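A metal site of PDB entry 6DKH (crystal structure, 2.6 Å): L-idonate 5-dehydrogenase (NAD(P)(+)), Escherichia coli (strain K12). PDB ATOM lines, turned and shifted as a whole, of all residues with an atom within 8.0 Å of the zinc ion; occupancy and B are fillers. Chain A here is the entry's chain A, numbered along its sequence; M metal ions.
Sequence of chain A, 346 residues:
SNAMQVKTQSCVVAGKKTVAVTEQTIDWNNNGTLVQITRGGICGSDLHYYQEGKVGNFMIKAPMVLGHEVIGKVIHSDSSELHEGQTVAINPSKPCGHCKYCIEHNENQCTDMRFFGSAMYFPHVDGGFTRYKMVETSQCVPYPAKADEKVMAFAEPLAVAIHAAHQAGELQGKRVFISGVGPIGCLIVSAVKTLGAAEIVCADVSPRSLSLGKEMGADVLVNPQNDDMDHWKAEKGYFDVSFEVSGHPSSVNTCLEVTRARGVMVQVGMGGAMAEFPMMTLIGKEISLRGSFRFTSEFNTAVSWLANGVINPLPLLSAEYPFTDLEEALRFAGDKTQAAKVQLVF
The zinc ion is bound by the side-chain sulfur (SG) of Cys 110 (2.3 Å), the side-chain sulfur (SG) of Cys 96 (2.4 Å), the side-chain sulfur (SG) of Cys 102 (2.4 Å) and the side-chain sulfur (SG) of Cys 99 (2.4 Å).
Of the 18 residues printed, 4 come within 4 Å of the zinc ion.
O of Asp 112 lies close to SG of Cys 110 (3.2 Å).
The side-chain sulfur of Cys 96 lies close to the backbone NH of His 98, at 3.7 Å.
SG of Cys 99 lies close to N of Tyr 101, 3.4 Å away.
N of Met 113 lies close to SG of Cys 110 (3.8 Å).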
ATOM      1  N   LYS A  94      14.504  22.795  -7.033  1.00  0.00           N
ATOM      2  CA  LYS A  94      15.877  22.613  -6.567  1.00  0.00           C
ATOM      3  C   LYS A  94      16.078  21.134  -6.266  1.00  0.00           C
ATOM      4  O   LYS A  94      15.857  20.671  -5.133  1.00  0.00           O
ATOM      5  CB  LYS A  94      16.184  23.465  -5.329  1.00  0.00           C
ATOM      6  CG  LYS A  94      17.669  23.492  -5.010  1.00  0.00           C
ATOM      7  CD  LYS A  94      17.951  23.426  -3.512  1.00  0.00           C
ATOM      8  CE  LYS A  94      19.440  23.236  -3.273  1.00  0.00           C
ATOM      9  NZ  LYS A  94      19.801  23.243  -1.835  1.00  0.00           N
ATOM     10  N   PRO A  95      16.481  20.355  -7.261  1.00  0.00           N
ATOM     11  CA  PRO A  95      16.729  18.935  -7.032  1.00  0.00           C
ATOM     12  C   PRO A  95      18.117  18.713  -6.451  1.00  0.00           C
ATOM     13  O   PRO A  95      18.995  19.573  -6.494  1.00  0.00           O
ATOM     14  CB  PRO A  95      16.628  18.330  -8.435  1.00  0.00           C
ATOM     15  CG  PRO A  95      17.125  19.441  -9.319  1.00  0.00           C
ATOM     16  CD  PRO A  95      16.665  20.730  -8.680  1.00  0.00           C
ATOM     17  N   CYS A  96      18.302  17.516  -5.880  1.00  0.00           N
ATOM     18  CA  CYS A  96      19.626  17.105  -5.447  1.00  0.00           C
ATOM     19  C   CYS A  96      20.426  16.644  -6.677  1.00  0.00           C
ATOM     20  O   CYS A  96      19.939  16.651  -7.811  1.00  0.00           O
ATOM     21  CB  CYS A  96      19.535  16.003  -4.392  1.00  0.00           C
ATOM     22  SG  CYS A  96      19.049  14.397  -5.044  1.00  0.00           S
ATOM     23  N   GLY A  97      21.668  16.260  -6.446  1.00  0.00           N
ATOM     24  CA  GLY A  97      22.510  15.795  -7.535  1.00  0.00           C
ATOM     25  C   GLY A  97      23.022  14.384  -7.356  1.00  0.00           C
ATOM     26  O   GLY A  97      24.009  13.999  -7.989  1.00  0.00           O
ATOM     27  N   HIS A  98      22.359  13.598  -6.507  1.00  0.00           N
ATOM     28  CA  HIS A  98      22.877  12.271  -6.165  1.00  0.00           C
ATOM     29  C   HIS A  98      21.827  11.162  -6.147  1.00  0.00           C
ATOM     30  O   HIS A  98      22.215   9.998  -6.018  1.00  0.00           O
ATOM     31  CB  HIS A  98      23.570  12.312  -4.799  1.00  0.00           C
ATOM     32  CG  HIS A  98      22.729  12.928  -3.719  1.00  0.00           C
ATOM     33  ND1 HIS A  98      21.730  12.236  -3.075  1.00  0.00           N
ATOM     34  CD2 HIS A  98      22.734  14.180  -3.190  1.00  0.00           C
ATOM     35  CE1 HIS A  98      21.152  13.031  -2.186  1.00  0.00           C
ATOM     36  NE2 HIS A  98      21.742  14.208  -2.232  1.00  0.00           N
ATOM     37  N   CYS A  99      20.543  11.470  -6.281  1.00  0.00           N
ATOM     38  CA  CYS A  99      19.521  10.431  -6.159  1.00  0.00           C
ATOM     39  C   CYS A  99      19.418   9.642  -7.463  1.00  0.00           C
ATOM     40  O   CYS A  99      20.117   9.897  -8.454  1.00  0.00           O
ATOM     41  CB  CYS A  99      18.175  11.035  -5.794  1.00  0.00           C
ATOM     42  SG  CYS A  99      17.163  11.537  -7.200  1.00  0.00           S
ATOM     43  N   LYS A 100      18.519   8.656  -7.462  1.00  0.00           N
ATOM     44  CA  LYS A 100      18.399   7.748  -8.596  1.00  0.00           C
ATOM     45  C   LYS A 100      17.888   8.469  -9.837  1.00  0.00           C
ATOM     46  O   LYS A 100      18.473   8.344 -10.917  1.00  0.00           O
ATOM     47  CB  LYS A 100      17.481   6.578  -8.224  1.00  0.00           C
ATOM     48  CG  LYS A 100      17.321   5.521  -9.300  1.00  0.00           C
ATOM     49  CD  LYS A 100      16.467   4.367  -8.792  1.00  0.00           C
ATOM     50  CE  LYS A 100      15.107   4.859  -8.308  1.00  0.00           C
ATOM     51  NZ  LYS A 100      14.263   3.746  -7.800  1.00  0.00           N
ATOM     52  N   TYR A 101      16.808   9.230  -9.698  1.00  0.00           N
ATOM     53  CA  TYR A 101      16.199   9.900 -10.834  1.00  0.00           C
ATOM     54  C   TYR A 101      16.968  11.153 -11.266  1.00  0.00           C
ATOM     55  O   TYR A 101      16.884  11.545 -12.434  1.00  0.00           O
ATOM     56  CB  TYR A 101      14.746  10.259 -10.523  1.00  0.00           C
ATOM     57  CG  TYR A 101      13.925   9.085 -10.057  1.00  0.00           C
ATOM     58  CD1 TYR A 101      13.435   8.153 -10.953  1.00  0.00           C
ATOM     59  CD2 TYR A 101      13.656   8.897  -8.705  1.00  0.00           C
ATOM     60  CE1 TYR A 101      12.688   7.062 -10.533  1.00  0.00           C
ATOM     61  CE2 TYR A 101      12.910   7.819  -8.263  1.00  0.00           C
ATOM     62  CZ  TYR A 101      12.430   6.906  -9.181  1.00  0.00           C
ATOM     63  OH  TYR A 101      11.696   5.827  -8.759  1.00  0.00           O
ATOM     64  N   CYS A 102      17.713  11.786 -10.359  1.00  0.00           N
ATOM     65  CA  CYS A 102      18.479  12.961 -10.743  1.00  0.00           C
ATOM     66  C   CYS A 102      19.702  12.602 -11.564  1.00  0.00           C
ATOM     67  O   CYS A 102      20.106  13.362 -12.448  1.00  0.00           O
ATOM     68  CB  CYS A 102      18.889  13.761  -9.515  1.00  0.00           C
ATOM     69  SG  CYS A 102      17.594  14.818  -8.840  1.00  0.00           S
ATOM     70  N   ILE A 103      20.317  11.450 -11.283  1.00  0.00           N
ATOM     71  CA  ILE A 103      21.468  11.016 -12.072  1.00  0.00           C
ATOM     72  C   ILE A 103      21.051  10.674 -13.489  1.00  0.00           C
ATOM     73  O   ILE A 103      21.779  10.943 -14.452  1.00  0.00           O
ATOM     74  CB  ILE A 103      22.170   9.835 -11.378  1.00  0.00           C
ATOM     75  CG1 ILE A 103      22.831  10.302 -10.073  1.00  0.00           C
ATOM     76  CG2 ILE A 103      23.202   9.200 -12.290  1.00  0.00           C
ATOM     77  CD1 ILE A 103      23.864  11.385 -10.268  1.00  0.00           C
ATOM     78  N   ASN A 106      16.145  12.759 -14.671  1.00  0.00           N
ATOM     79  CA  ASN A 106      14.712  12.853 -14.419  1.00  0.00           C
ATOM     80  C   ASN A 106      14.470  13.601 -13.117  1.00  0.00           C
ATOM     81  O   ASN A 106      13.755  13.114 -12.240  1.00  0.00           O
ATOM     82  CB  ASN A 106      14.071  11.460 -14.371  1.00  0.00           C
ATOM     83  CG  ASN A 106      14.177  10.710 -15.682  1.00  0.00           C
ATOM     84  OD1 ASN A 106      14.073  11.299 -16.757  1.00  0.00           O
ATOM     85  ND2 ASN A 106      14.386   9.405 -15.599  1.00  0.00           N
ATOM     86  N   GLU A 107      15.084  14.785 -12.977  1.00  0.00           N
ATOM     87  CA  GLU A 107      15.042  15.517 -11.716  1.00  0.00           C
ATOM     88  C   GLU A 107      13.647  15.959 -11.310  1.00  0.00           C
ATOM     89  O   GLU A 107      13.455  16.337 -10.156  1.00  0.00           O
ATOM     90  CB  GLU A 107      15.981  16.724 -11.773  1.00  0.00           C
ATOM     91  CG  GLU A 107      16.339  17.198 -13.173  1.00  0.00           C
ATOM     92  CD  GLU A 107      17.651  16.621 -13.663  1.00  0.00           C
ATOM     93  OE1 GLU A 107      18.512  16.302 -12.818  1.00  0.00           O
ATOM     94  OE2 GLU A 107      17.819  16.487 -14.895  1.00  0.00           O
ATOM     95  N   ASN A 108      12.671  15.939 -12.226  1.00  0.00           N
ATOM     96  CA  ASN A 108      11.306  16.223 -11.818  1.00  0.00           C
ATOM     97  C   ASN A 108      10.757  15.151 -10.883  1.00  0.00           C
ATOM     98  O   ASN A 108       9.814  15.419 -10.131  1.00  0.00           O
ATOM     99  CB  ASN A 108      10.388  16.365 -13.043  1.00  0.00           C
ATOM    100  CG  ASN A 108      10.117  15.038 -13.714  1.00  0.00           C
ATOM    101  OD1 ASN A 108      10.977  14.154 -13.757  1.00  0.00           O
ATOM    102  ND2 ASN A 108       8.912  14.887 -14.253  1.00  0.00           N
ATOM    103  N   GLN A 109      11.324  13.950 -10.922  1.00  0.00           N
ATOM    104  CA  GLN A 109      10.977  12.864 -10.006  1.00  0.00           C
ATOM    105  C   GLN A 109      11.998  12.714  -8.880  1.00  0.00           C
ATOM    106  O   GLN A 109      12.192  11.614  -8.364  1.00  0.00           O
ATOM    107  CB  GLN A 109      10.842  11.551 -10.777  1.00  0.00           C
ATOM    108  CG  GLN A 109       9.747  11.551 -11.823  1.00  0.00           C
ATOM    109  CD  GLN A 109       8.357  11.465 -11.217  1.00  0.00           C
ATOM    110  OE1 GLN A 109       8.200  11.184 -10.030  1.00  0.00           O
ATOM    111  NE2 GLN A 109       7.338  11.711 -12.035  1.00  0.00           N
ATOM    112  N   CYS A 110      12.658  13.810  -8.507  1.00  0.00           N
ATOM    113  CA  CYS A 110      13.690  13.743  -7.471  1.00  0.00           C
ATOM    114  C   CYS A 110      13.106  13.284  -6.145  1.00  0.00           C
ATOM    115  O   CYS A 110      12.040  13.746  -5.723  1.00  0.00           O
ATOM    116  CB  CYS A 110      14.359  15.115  -7.308  1.00  0.00           C
ATOM    117  SG  CYS A 110      15.574  15.180  -5.978  1.00  0.00           S
ATOM    118  N   THR A 111      13.823  12.374  -5.485  1.00  0.00           N
ATOM    119  CA  THR A 111      13.378  11.895  -4.184  1.00  0.00           C
ATOM    120  C   THR A 111      13.431  13.000  -3.142  1.00  0.00           C
ATOM    121  O   THR A 111      12.522  13.127  -2.309  1.00  0.00           O
ATOM    122  CB  THR A 111      14.246  10.708  -3.750  1.00  0.00           C
ATOM    123  OG1 THR A 111      14.028   9.610  -4.641  1.00  0.00           O
ATOM    124  CG2 THR A 111      13.896  10.266  -2.335  1.00  0.00           C
ATOM    125  N   ASP A 112      14.476  13.827  -3.167  1.00  0.00           N
ATOM    126  CA  ASP A 112      14.647  14.925  -2.221  1.00  0.00           C
ATOM    127  C   ASP A 112      14.494  16.239  -2.996  1.00  0.00           C
ATOM    128  O   ASP A 112      15.477  16.939  -3.273  1.00  0.00           O
ATOM    129  CB  ASP A 112      16.003  14.821  -1.517  1.00  0.00           C
ATOM    130  CG  ASP A 112      16.097  15.723  -0.294  1.00  0.00           C
ATOM    131  OD1 ASP A 112      15.102  16.396   0.029  1.00  0.00           O
ATOM    132  OD2 ASP A 112      17.171  15.759   0.332  1.00  0.00           O
ATOM    133  N   MET A 113      13.253  16.574  -3.340  1.00  0.00           N
ATOM    134  CA  MET A 113      12.940  17.707  -4.190  1.00  0.00           C
ATOM    135  C   MET A 113      12.367  18.850  -3.364  1.00  0.00           C
ATOM    136  O   MET A 113      11.576  18.632  -2.440  1.00  0.00           O
ATOM    137  CB  MET A 113      11.940  17.309  -5.278  1.00  0.00           C
ATOM    138  CG  MET A 113      11.193  18.479  -5.931  1.00  0.00           C
ATOM    139  SD  MET A 113      12.293  19.660  -6.741  1.00  0.00           S
ATOM    140  CE  MET A 113      12.735  18.765  -8.221  1.00  0.00           C
HETATM  141 ZN    ZN M   1      17.401  13.909  -6.651  1.00  0.00          ZN
